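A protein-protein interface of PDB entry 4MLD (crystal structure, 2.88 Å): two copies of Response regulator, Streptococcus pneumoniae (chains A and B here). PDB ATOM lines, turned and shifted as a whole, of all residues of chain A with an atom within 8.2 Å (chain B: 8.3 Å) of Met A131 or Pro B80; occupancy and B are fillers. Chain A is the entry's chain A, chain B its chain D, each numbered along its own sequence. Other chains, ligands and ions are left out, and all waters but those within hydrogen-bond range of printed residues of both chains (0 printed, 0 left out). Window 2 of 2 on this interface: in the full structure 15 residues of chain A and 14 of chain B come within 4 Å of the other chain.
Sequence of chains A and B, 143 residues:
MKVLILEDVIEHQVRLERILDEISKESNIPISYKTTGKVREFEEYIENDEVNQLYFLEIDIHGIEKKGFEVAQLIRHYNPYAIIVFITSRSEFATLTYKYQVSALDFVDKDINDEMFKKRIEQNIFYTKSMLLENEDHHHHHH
Ser B103 touches its own counterpart, Ser A103. Of the 6 pairs that touch across the chains among the printed residues, 1 has its exchanged pair printed and touching as well.
Ser B103 touches Ser A103 (O to CB, 3.3 Å). Gln B101 touches Leu A105. Ser B103 touches Leu A105 (OG to CA, 3.97 Å). Tyr A127 touches Arg B76 (OH to CD, 3.6 Å). Gln B101 touches Tyr A127. Met A131 touches Pro B80 (CE to CB, 3.6 Å).
The backbone carbonyl oxygen of Tyr A127 is in hydrogen-bond range of the side-chain hydroxyl of Ser A130, 2.8 Å away. The guanidinium group (NH1) of Arg B76 lies within hydrogen-bond range of the backbone carbonyl oxygen (O) of Pro B80 (2.4 Å). O of Ala B82 sits at hydrogen-bond distance from NH1 of Arg B76 (3.1 Å). NH2 of Arg B76 sits at hydrogen-bond distance from O of Ser B103 (3.4 Å).
Printed residues of chain B that touch a printed residue of chain A: Arg B76, Pro B80, Gln B101 and Ser B103. Hydrophobic or aromatic side chains of chain B within 4 Å of the printed part of chain A: Pro B80. Of the 17 printed residues of chain A, 4 touch a printed residue of chain B. Among the printed residues, 6 pairs touch across the chains.
Printed residues of chain B within 4 Å of Ser A103: Ser B103 (3.3 Å). Of the printed residues of chain A, Arg B76 touches Tyr A127 (3.6 Å). Pro B80 touches one residue of chain A. Printed residues of chain A within 4 Å of Gln B101: Leu A105 (3.6 Å) and Tyr A127 (3.4 Å). The nearest residue of chain B that does not touch Met A131 is Arg B76 (5.4 Å). The nearest printed residue of chain B that does not touch Ser A103 is Arg B76 (6.0 Å).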
ATOM      1  N   MET A   1     -29.299 -10.122 -34.082  1.00  0.00           N
ATOM      2  CA  MET A   1     -29.434  -9.134 -33.019  1.00  0.00           C
ATOM      3  C   MET A   1     -30.854  -8.575 -32.956  1.00  0.00           C
ATOM      4  O   MET A   1     -31.543  -8.488 -33.973  1.00  0.00           O
ATOM      5  CB  MET A   1     -28.425  -7.995 -33.207  1.00  0.00           C
ATOM      6  CG  MET A   1     -28.626  -7.178 -34.475  1.00  0.00           C
ATOM      7  SD  MET A   1     -27.568  -5.717 -34.559  1.00  0.00           S
ATOM      8  CE  MET A   1     -25.941  -6.468 -34.582  1.00  0.00           C
ATOM      9  N   GLN A  53     -30.274  -5.426 -27.563  1.00  0.00           N
ATOM     10  CA  GLN A  53     -28.978  -4.767 -27.429  1.00  0.00           C
ATOM     11  C   GLN A  53     -29.028  -3.314 -27.893  1.00  0.00           C
ATOM     12  O   GLN A  53     -28.429  -2.437 -27.274  1.00  0.00           O
ATOM     13  CB  GLN A  53     -27.900  -5.517 -28.218  1.00  0.00           C
ATOM     14  CG  GLN A  53     -27.584  -6.915 -27.705  1.00  0.00           C
ATOM     15  CD  GLN A  53     -28.507  -7.975 -28.277  1.00  0.00           C
ATOM     16  OE1 GLN A  53     -29.381  -7.682 -29.094  1.00  0.00           O
ATOM     17  NE2 GLN A  53     -28.312  -9.219 -27.852  1.00  0.00           N
ATOM     18  N   PRO A  80     -28.068  -2.115 -18.191  1.00  0.00           N
ATOM     19  CA  PRO A  80     -26.927  -1.194 -18.196  1.00  0.00           C
ATOM     20  C   PRO A  80     -25.974  -1.431 -19.363  1.00  0.00           C
ATOM     21  O   PRO A  80     -25.129  -0.580 -19.642  1.00  0.00           O
ATOM     22  CB  PRO A  80     -26.231  -1.489 -16.863  1.00  0.00           C
ATOM     23  CG  PRO A  80     -26.646  -2.877 -16.514  1.00  0.00           C
ATOM     24  CD  PRO A  80     -28.045  -3.023 -17.030  1.00  0.00           C
ATOM     25  N   TYR A  81     -26.112  -2.570 -20.034  1.00  0.00           N
ATOM     26  CA  TYR A  81     -25.252  -2.901 -21.165  1.00  0.00           C
ATOM     27  C   TYR A  81     -25.902  -2.497 -22.482  1.00  0.00           C
ATOM     28  O   TYR A  81     -25.393  -2.803 -23.559  1.00  0.00           O
ATOM     29  CB  TYR A  81     -24.948  -4.399 -21.180  1.00  0.00           C
ATOM     30  CG  TYR A  81     -24.542  -4.950 -19.834  1.00  0.00           C
ATOM     31  CD1 TYR A  81     -23.286  -4.684 -19.304  1.00  0.00           C
ATOM     32  CD2 TYR A  81     -25.414  -5.738 -19.093  1.00  0.00           C
ATOM     33  CE1 TYR A  81     -22.911  -5.184 -18.073  1.00  0.00           C
ATOM     34  CE2 TYR A  81     -25.047  -6.244 -17.861  1.00  0.00           C
ATOM     35  CZ  TYR A  81     -23.793  -5.964 -17.356  1.00  0.00           C
ATOM     36  OH  TYR A  81     -23.422  -6.465 -16.128  1.00  0.00           O
ATOM     37  N   ILE A  83     -27.161  -0.517 -25.710  1.00  0.00           N
ATOM     38  CA  ILE A  83     -26.705   0.512 -26.634  1.00  0.00           C
ATOM     39  C   ILE A  83     -27.880   1.402 -27.010  1.00  0.00           C
ATOM     40  O   ILE A  83     -28.814   0.964 -27.677  1.00  0.00           O
ATOM     41  CB  ILE A  83     -26.116  -0.095 -27.921  1.00  0.00           C
ATOM     42  CG1 ILE A  83     -25.021  -1.109 -27.590  1.00  0.00           C
ATOM     43  CG2 ILE A  83     -25.575   1.001 -28.830  1.00  0.00           C
ATOM     44  CD1 ILE A  83     -24.409  -1.758 -28.809  1.00  0.00           C
ATOM     45  N   SER A 103     -26.000   6.975 -21.826  1.00  0.00           N
ATOM     46  CA  SER A 103     -24.730   7.014 -22.536  1.00  0.00           C
ATOM     47  C   SER A 103     -24.973   6.667 -23.992  1.00  0.00           C
ATOM     48  O   SER A 103     -24.606   5.590 -24.461  1.00  0.00           O
ATOM     49  CB  SER A 103     -23.718   6.069 -21.891  1.00  0.00           C
ATOM     50  OG  SER A 103     -23.448   6.464 -20.555  1.00  0.00           O
ATOM     51  N   LEU A 105     -24.924   6.128 -27.817  1.00  0.00           N
ATOM     52  CA  LEU A 105     -23.889   5.870 -28.806  1.00  0.00           C
ATOM     53  C   LEU A 105     -23.912   6.963 -29.862  1.00  0.00           C
ATOM     54  O   LEU A 105     -22.867   7.455 -30.287  1.00  0.00           O
ATOM     55  CB  LEU A 105     -24.097   4.505 -29.462  1.00  0.00           C
ATOM     56  CG  LEU A 105     -23.094   4.143 -30.562  1.00  0.00           C
ATOM     57  CD1 LEU A 105     -21.688   4.016 -29.992  1.00  0.00           C
ATOM     58  CD2 LEU A 105     -23.512   2.868 -31.278  1.00  0.00           C
ATOM     59  N   ASN A 124     -24.188   2.360 -36.379  1.00  0.00           N
ATOM     60  CA  ASN A 124     -24.668   1.961 -35.064  1.00  0.00           C
ATOM     61  C   ASN A 124     -24.900   0.455 -34.978  1.00  0.00           C
ATOM     62  O   ASN A 124     -24.738  -0.146 -33.917  1.00  0.00           O
ATOM     63  CB  ASN A 124     -25.934   2.736 -34.693  1.00  0.00           C
ATOM     64  CG  ASN A 124     -25.720   4.239 -34.699  1.00  0.00           C
ATOM     65  OD1 ASN A 124     -24.593   4.718 -34.565  1.00  0.00           O
ATOM     66  ND2 ASN A 124     -26.802   4.991 -34.858  1.00  0.00           N
ATOM     67  N   ILE A 125     -25.265  -0.151 -36.101  1.00  0.00           N
ATOM     68  CA  ILE A 125     -25.491  -1.591 -36.161  1.00  0.00           C
ATOM     69  C   ILE A 125     -24.164  -2.351 -36.192  1.00  0.00           C
ATOM     70  O   ILE A 125     -24.012  -3.379 -35.527  1.00  0.00           O
ATOM     71  CB  ILE A 125     -26.376  -1.965 -37.373  1.00  0.00           C
ATOM     72  CG1 ILE A 125     -27.821  -1.537 -37.117  1.00  0.00           C
ATOM     73  CG2 ILE A 125     -26.317  -3.454 -37.657  1.00  0.00           C
ATOM     74  CD1 ILE A 125     -28.775  -1.933 -38.218  1.00  0.00           C
ATOM     75  N   PHE A 126     -23.213  -1.832 -36.967  1.00  0.00           N
ATOM     76  CA  PHE A 126     -21.859  -2.378 -37.021  1.00  0.00           C
ATOM     77  C   PHE A 126     -21.227  -2.362 -35.636  1.00  0.00           C
ATOM     78  O   PHE A 126     -20.667  -3.362 -35.189  1.00  0.00           O
ATOM     79  CB  PHE A 126     -20.991  -1.577 -37.996  1.00  0.00           C
ATOM     80  CG  PHE A 126     -21.389  -1.736 -39.441  1.00  0.00           C
ATOM     81  CD1 PHE A 126     -22.138  -2.834 -39.860  1.00  0.00           C
ATOM     82  CD2 PHE A 126     -21.004  -0.791 -40.385  1.00  0.00           C
ATOM     83  CE1 PHE A 126     -22.502  -2.978 -41.198  1.00  0.00           C
ATOM     84  CE2 PHE A 126     -21.365  -0.928 -41.717  1.00  0.00           C
ATOM     85  CZ  PHE A 126     -22.113  -2.021 -42.124  1.00  0.00           C
ATOM     86  N   TYR A 127     -21.327  -1.214 -34.968  1.00  0.00           N
ATOM     87  CA  TYR A 127     -20.830  -1.057 -33.608  1.00  0.00           C
ATOM     88  C   TYR A 127     -21.439  -2.107 -32.687  1.00  0.00           C
ATOM     89  O   TYR A 127     -20.760  -2.657 -31.817  1.00  0.00           O
ATOM     90  CB  TYR A 127     -21.157   0.343 -33.079  1.00  0.00           C
ATOM     91  CG  TYR A 127     -20.649   0.608 -31.677  1.00  0.00           C
ATOM     92  CD1 TYR A 127     -19.432   1.241 -31.469  1.00  0.00           C
ATOM     93  CD2 TYR A 127     -21.388   0.225 -30.562  1.00  0.00           C
ATOM     94  CE1 TYR A 127     -18.962   1.481 -30.190  1.00  0.00           C
ATOM     95  CE2 TYR A 127     -20.928   0.460 -29.284  1.00  0.00           C
ATOM     96  CZ  TYR A 127     -19.716   1.087 -29.102  1.00  0.00           C
ATOM     97  OH  TYR A 127     -19.262   1.323 -27.825  1.00  0.00           O
ATOM     98  N   THR A 128     -22.726  -2.371 -32.883  1.00  0.00           N
ATOM     99  CA  THR A 128     -23.446  -3.347 -32.082  1.00  0.00           C
ATOM    100  C   THR A 128     -22.881  -4.751 -32.275  1.00  0.00           C
ATOM    101  O   THR A 128     -22.635  -5.461 -31.301  1.00  0.00           O
ATOM    102  CB  THR A 128     -24.948  -3.349 -32.424  1.00  0.00           C
ATOM    103  OG1 THR A 128     -25.482  -2.028 -32.264  1.00  0.00           O
ATOM    104  CG2 THR A 128     -25.698  -4.310 -31.517  1.00  0.00           C
ATOM    105  N   LYS A 129     -22.668  -5.146 -33.529  1.00  0.00           N
ATOM    106  CA  LYS A 129     -22.175  -6.489 -33.833  1.00  0.00           C
ATOM    107  C   LYS A 129     -20.778  -6.728 -33.270  1.00  0.00           C
ATOM    108  O   LYS A 129     -20.491  -7.799 -32.736  1.00  0.00           O
ATOM    109  CB  LYS A 129     -22.177  -6.753 -35.341  1.00  0.00           C
ATOM    110  CG  LYS A 129     -21.788  -8.184 -35.703  1.00  0.00           C
ATOM    111  CD  LYS A 129     -21.880  -8.434 -37.201  1.00  0.00           C
ATOM    112  CE  LYS A 129     -20.841  -7.634 -37.967  1.00  0.00           C
ATOM    113  NZ  LYS A 129     -19.450  -8.038 -37.617  1.00  0.00           N
ATOM    114  N   SER A 130     -19.914  -5.727 -33.401  1.00  0.00           N
ATOM    115  CA  SER A 130     -18.550  -5.828 -32.899  1.00  0.00           C
ATOM    116  C   SER A 130     -18.554  -5.918 -31.378  1.00  0.00           C
ATOM    117  O   SER A 130     -17.765  -6.654 -30.787  1.00  0.00           O
ATOM    118  CB  SER A 130     -17.722  -4.628 -33.359  1.00  0.00           C
ATOM    119  OG  SER A 130     -18.287  -3.414 -32.895  1.00  0.00           O
ATOM    120  N   MET A 131     -19.459  -5.170 -30.753  1.00  0.00           N
ATOM    121  CA  MET A 131     -19.588  -5.167 -29.300  1.00  0.00           C
ATOM    122  C   MET A 131     -20.262  -6.437 -28.785  1.00  0.00           C
ATOM    123  O   MET A 131     -20.303  -6.686 -27.580  1.00  0.00           O
ATOM    124  CB  MET A 131     -20.346  -3.925 -28.832  1.00  0.00           C
ATOM    125  CG  MET A 131     -19.488  -2.673 -28.769  1.00  0.00           C
ATOM    126  SD  MET A 131     -18.234  -2.803 -27.485  1.00  0.00           S
ATOM    127  CE  MET A 131     -19.271  -3.188 -26.078  1.00  0.00           C
ATOM    128  N   LEU A 132     -20.785  -7.234 -29.713  1.00  0.00           N
ATOM    129  CA  LEU A 132     -21.336  -8.545 -29.394  1.00  0.00           C
ATOM    130  C   LEU A 132     -20.226  -9.596 -29.398  1.00  0.00           C
ATOM    131  O   LEU A 132     -20.500 -10.797 -29.461  1.00  0.00           O
ATOM    132  CB  LEU A 132     -22.417  -8.923 -30.410  1.00  0.00           C
ATOM    133  CG  LEU A 132     -23.881  -8.808 -29.973  1.00  0.00           C
ATOM    134  CD1 LEU A 132     -24.105  -7.602 -29.075  1.00  0.00           C
ATOM    135  CD2 LEU A 132     -24.799  -8.760 -31.187  1.00  0.00           C
ATOM    136  N   LEU A 133     -18.981  -9.127 -29.318  1.00  0.00           N
ATOM    137  CA  LEU A 133     -17.789  -9.976 -29.402  1.00  0.00           C
ATOM    138  C   LEU A 133     -17.729 -10.735 -30.724  1.00  0.00           C
ATOM    139  O   LEU A 133     -17.532 -10.139 -31.785  1.00  0.00           O
ATOM    140  CB  LEU A 133     -17.679 -10.938 -28.207  1.00  0.00           C
ATOM    141  CG  LEU A 133     -17.142 -10.417 -26.865  1.00  0.00           C
ATOM    142  CD1 LEU A 133     -18.093  -9.420 -26.223  1.00  0.00           C
ATOM    143  CD2 LEU A 133     -16.853 -11.564 -25.901  1.00  0.00           C
ATOM    144  N   GLU B  50      -7.808  -2.249 -15.545  1.00  0.00           N
ATOM    145  CA  GLU B  50      -9.130  -1.672 -15.749  1.00  0.00           C
ATOM    146  C   GLU B  50     -10.035  -1.777 -14.519  1.00  0.00           C
ATOM    147  O   GLU B  50     -11.229  -2.052 -14.643  1.00  0.00           O
ATOM    148  CB  GLU B  50      -9.823  -2.303 -16.962  1.00  0.00           C
ATOM    149  CG  GLU B  50      -9.072  -2.164 -18.282  1.00  0.00           C
ATOM    150  CD  GLU B  50      -8.997  -0.731 -18.790  1.00  0.00           C
ATOM    151  OE1 GLU B  50      -9.659   0.160 -18.213  1.00  0.00           O
ATOM    152  OE2 GLU B  50      -8.273  -0.497 -19.781  1.00  0.00           O
ATOM    153  N   GLN B  53     -13.196   2.655 -13.185  1.00  0.00           N
ATOM    154  CA  GLN B  53     -14.553   2.730 -13.698  1.00  0.00           C
ATOM    155  C   GLN B  53     -14.778   4.110 -14.294  1.00  0.00           C
ATOM    156  O   GLN B  53     -15.465   4.259 -15.302  1.00  0.00           O
ATOM    157  CB  GLN B  53     -15.567   2.484 -12.580  1.00  0.00           C
ATOM    158  CG  GLN B  53     -15.221   1.334 -11.645  1.00  0.00           C
ATOM    159  CD  GLN B  53     -14.294   1.751 -10.518  1.00  0.00           C
ATOM    160  OE1 GLN B  53     -13.880   2.908 -10.435  1.00  0.00           O
ATOM    161  NE2 GLN B  53     -13.960   0.807  -9.646  1.00  0.00           N
ATOM    162  N   GLN B  73     -11.499   6.551 -27.156  1.00  0.00           N
ATOM    163  CA  GLN B  73     -11.769   5.420 -28.040  1.00  0.00           C
ATOM    164  C   GLN B  73     -10.956   4.206 -27.612  1.00  0.00           C
ATOM    165  O   GLN B  73     -11.423   3.070 -27.687  1.00  0.00           O
ATOM    166  CB  GLN B  73     -11.460   5.778 -29.495  1.00  0.00           C
ATOM    167  CG  GLN B  73     -12.459   6.730 -30.134  1.00  0.00           C
ATOM    168  CD  GLN B  73     -12.146   7.015 -31.591  1.00  0.00           C
ATOM    169  OE1 GLN B  73     -11.015   7.350 -31.942  1.00  0.00           O
ATOM    170  NE2 GLN B  73     -13.148   6.875 -32.450  1.00  0.00           N
ATOM    171  N   LEU B  74      -9.733   4.464 -27.159  1.00  0.00           N
ATOM    172  CA  LEU B  74      -8.865   3.421 -26.637  1.00  0.00           C
ATOM    173  C   LEU B  74      -9.457   2.865 -25.343  1.00  0.00           C
ATOM    174  O   LEU B  74      -9.479   1.652 -25.129  1.00  0.00           O
ATOM    175  CB  LEU B  74      -7.464   3.986 -26.396  1.00  0.00           C
ATOM    176  CG  LEU B  74      -6.287   3.021 -26.255  1.00  0.00           C
ATOM    177  CD1 LEU B  74      -5.000   3.714 -26.674  1.00  0.00           C
ATOM    178  CD2 LEU B  74      -6.166   2.513 -24.832  1.00  0.00           C
ATOM    179  N   ILE B  75      -9.937   3.764 -24.488  1.00  0.00           N
ATOM    180  CA  ILE B  75     -10.592   3.380 -23.242  1.00  0.00           C
ATOM    181  C   ILE B  75     -11.828   2.536 -23.524  1.00  0.00           C
ATOM    182  O   ILE B  75     -12.022   1.480 -22.921  1.00  0.00           O
ATOM    183  CB  ILE B  75     -11.017   4.616 -22.433  1.00  0.00           C
ATOM    184  CG1 ILE B  75      -9.794   5.453 -22.064  1.00  0.00           C
ATOM    185  CG2 ILE B  75     -11.772   4.203 -21.179  1.00  0.00           C
ATOM    186  CD1 ILE B  75     -10.131   6.759 -21.397  1.00  0.00           C
ATOM    187  N   ARG B  76     -12.656   3.014 -24.447  1.00  0.00           N
ATOM    188  CA  ARG B  76     -13.861   2.301 -24.851  1.00  0.00           C
ATOM    189  C   ARG B  76     -13.522   0.910 -25.374  1.00  0.00           C
ATOM    190  O   ARG B  76     -14.234  -0.057 -25.101  1.00  0.00           O
ATOM    191  CB  ARG B  76     -14.612   3.094 -25.922  1.00  0.00           C
ATOM    192  CG  ARG B  76     -15.882   2.421 -26.414  1.00  0.00           C
ATOM    193  CD  ARG B  76     -16.827   2.144 -25.259  1.00  0.00           C
ATOM    194  NE  ARG B  76     -17.224   3.373 -24.579  1.00  0.00           N
ATOM    195  CZ  ARG B  76     -17.653   3.425 -23.323  1.00  0.00           C
ATOM    196  NH1 ARG B  76     -17.733   2.315 -22.602  1.00  0.00           N
ATOM    197  NH2 ARG B  76     -17.994   4.587 -22.786  1.00  0.00           N
ATOM    198  N   HIS B  77     -12.425   0.818 -26.117  1.00  0.00           N
ATOM    199  CA  HIS B  77     -11.994  -0.442 -26.711  1.00  0.00           C
ATOM    200  C   HIS B  77     -11.564  -1.462 -25.658  1.00  0.00           C
ATOM    201  O   HIS B  77     -12.084  -2.578 -25.618  1.00  0.00           O
ATOM    202  CB  HIS B  77     -10.853  -0.201 -27.702  1.00  0.00           C
ATOM    203  CG  HIS B  77     -10.338  -1.451 -28.344  1.00  0.00           C
ATOM    204  ND1 HIS B  77      -9.158  -2.051 -27.961  1.00  0.00           N
ATOM    205  CD2 HIS B  77     -10.844  -2.216 -29.340  1.00  0.00           C
ATOM    206  CE1 HIS B  77      -8.957  -3.131 -28.696  1.00  0.00           C
ATOM    207  NE2 HIS B  77      -9.966  -3.253 -29.539  1.00  0.00           N
ATOM    208  N   TYR B  78     -10.613  -1.078 -24.814  1.00  0.00           N
ATOM    209  CA  TYR B  78     -10.124  -1.965 -23.763  1.00  0.00           C
ATOM    210  C   TYR B  78     -11.199  -2.251 -22.728  1.00  0.00           C
ATOM    211  O   TYR B  78     -11.299  -3.365 -22.215  1.00  0.00           O
ATOM    212  CB  TYR B  78      -8.892  -1.369 -23.081  1.00  0.00           C
ATOM    213  CG  TYR B  78      -7.588  -1.780 -23.721  1.00  0.00           C
ATOM    214  CD1 TYR B  78      -7.309  -3.116 -23.977  1.00  0.00           C
ATOM    215  CD2 TYR B  78      -6.642  -0.832 -24.080  1.00  0.00           C
ATOM    216  CE1 TYR B  78      -6.119  -3.496 -24.564  1.00  0.00           C
ATOM    217  CE2 TYR B  78      -5.451  -1.201 -24.670  1.00  0.00           C
ATOM    218  CZ  TYR B  78      -5.193  -2.534 -24.909  1.00  0.00           C
ATOM    219  OH  TYR B  78      -4.005  -2.903 -25.497  1.00  0.00           O
ATOM    220  N   ASN B  79     -12.001  -1.239 -22.422  1.00  0.00           N
ATOM    221  CA  ASN B  79     -13.049  -1.387 -21.426  1.00  0.00           C
ATOM    222  C   ASN B  79     -14.386  -0.845 -21.920  1.00  0.00           C
ATOM    223  O   ASN B  79     -14.603   0.366 -21.937  1.00  0.00           O
ATOM    224  CB  ASN B  79     -12.639  -0.706 -20.117  1.00  0.00           C
ATOM    225  CG  ASN B  79     -13.380  -1.255 -18.915  1.00  0.00           C
ATOM    226  OD1 ASN B  79     -13.767  -0.510 -18.015  1.00  0.00           O
ATOM    227  ND2 ASN B  79     -13.588  -2.566 -18.898  1.00  0.00           N
ATOM    228  N   PRO B  80     -15.279  -1.750 -22.347  1.00  0.00           N
ATOM    229  CA  PRO B  80     -16.636  -1.370 -22.749  1.00  0.00           C
ATOM    230  C   PRO B  80     -17.417  -0.809 -21.567  1.00  0.00           C
ATOM    231  O   PRO B  80     -18.239   0.092 -21.735  1.00  0.00           O
ATOM    232  CB  PRO B  80     -17.250  -2.701 -23.194  1.00  0.00           C
ATOM    233  CG  PRO B  80     -16.089  -3.560 -23.554  1.00  0.00           C
ATOM    234  CD  PRO B  80     -15.008  -3.176 -22.591  1.00  0.00           C
ATOM    235  N   TYR B  81     -17.145  -1.339 -20.379  1.00  0.00           N
ATOM    236  CA  TYR B  81     -17.863  -0.954 -19.168  1.00  0.00           C
ATOM    237  C   TYR B  81     -17.451   0.430 -18.681  1.00  0.00           C
ATOM    238  O   TYR B  81     -18.150   1.044 -17.875  1.00  0.00           O
ATOM    239  CB  TYR B  81     -17.601  -1.961 -18.044  1.00  0.00           C
ATOM    240  CG  TYR B  81     -17.923  -3.400 -18.379  1.00  0.00           C
ATOM    241  CD1 TYR B  81     -17.376  -4.439 -17.636  1.00  0.00           C
ATOM    242  CD2 TYR B  81     -18.776  -3.722 -19.427  1.00  0.00           C
ATOM    243  CE1 TYR B  81     -17.665  -5.756 -17.930  1.00  0.00           C
ATOM    244  CE2 TYR B  81     -19.069  -5.038 -19.730  1.00  0.00           C
ATOM    245  CZ  TYR B  81     -18.511  -6.051 -18.978  1.00  0.00           C
ATOM    246  OH  TYR B  81     -18.802  -7.362 -19.273  1.00  0.00           O
ATOM    247  N   ALA B  82     -16.310   0.908 -19.164  1.00  0.00           N
ATOM    248  CA  ALA B  82     -15.723   2.156 -18.686  1.00  0.00           C
ATOM    249  C   ALA B  82     -16.649   3.361 -18.821  1.00  0.00           C
ATOM    250  O   ALA B  82     -17.196   3.624 -19.891  1.00  0.00           O
ATOM    251  CB  ALA B  82     -14.403   2.424 -19.396  1.00  0.00           C
ATOM    252  N   ILE B  83     -16.820   4.086 -17.721  1.00  0.00           N
ATOM    253  CA  ILE B  83     -17.569   5.334 -17.733  1.00  0.00           C
ATOM    254  C   ILE B  83     -16.640   6.465 -18.156  1.00  0.00           C
ATOM    255  O   ILE B  83     -15.577   6.662 -17.568  1.00  0.00           O
ATOM    256  CB  ILE B  83     -18.164   5.657 -16.350  1.00  0.00           C
ATOM    257  CG1 ILE B  83     -18.966   4.464 -15.825  1.00  0.00           C
ATOM    258  CG2 ILE B  83     -19.030   6.907 -16.418  1.00  0.00           C
ATOM    259  CD1 ILE B  83     -19.563   4.686 -14.455  1.00  0.00           C
ATOM    260  N   ILE B  84     -17.045   7.202 -19.184  1.00  0.00           N
ATOM    261  CA  ILE B  84     -16.205   8.250 -19.745  1.00  0.00           C
ATOM    262  C   ILE B  84     -16.915   9.597 -19.710  1.00  0.00           C
ATOM    263  O   ILE B  84     -17.949   9.778 -20.348  1.00  0.00           O
ATOM    264  CB  ILE B  84     -15.820   7.925 -21.202  1.00  0.00           C
ATOM    265  CG1 ILE B  84     -15.226   6.517 -21.294  1.00  0.00           C
ATOM    266  CG2 ILE B  84     -14.854   8.964 -21.746  1.00  0.00           C
ATOM    267  CD1 ILE B  84     -14.874   6.089 -22.702  1.00  0.00           C
ATOM    268  N   GLN B 101     -17.790   7.384 -31.506  1.00  0.00           N
ATOM    269  CA  GLN B 101     -18.458   6.176 -31.028  1.00  0.00           C
ATOM    270  C   GLN B 101     -18.127   5.828 -29.580  1.00  0.00           C
ATOM    271  O   GLN B 101     -18.262   4.676 -29.161  1.00  0.00           O
ATOM    272  CB  GLN B 101     -18.185   4.996 -31.965  1.00  0.00           C
ATOM    273  CG  GLN B 101     -18.880   5.114 -33.317  1.00  0.00           C
ATOM    274  CD  GLN B 101     -18.631   3.910 -34.202  1.00  0.00           C
ATOM    275  OE1 GLN B 101     -17.621   3.220 -34.060  1.00  0.00           O
ATOM    276  NE2 GLN B 101     -19.552   3.651 -35.123  1.00  0.00           N
ATOM    277  N   SER B 103     -19.324   6.251 -25.711  1.00  0.00           N
ATOM    278  CA  SER B 103     -20.622   6.455 -25.087  1.00  0.00           C
ATOM    279  C   SER B 103     -20.425   7.280 -23.834  1.00  0.00           C
ATOM    280  O   SER B 103     -20.621   6.790 -22.720  1.00  0.00           O
ATOM    281  CB  SER B 103     -21.296   5.125 -24.763  1.00  0.00           C
ATOM    282  OG  SER B 103     -21.552   4.399 -25.950  1.00  0.00           O
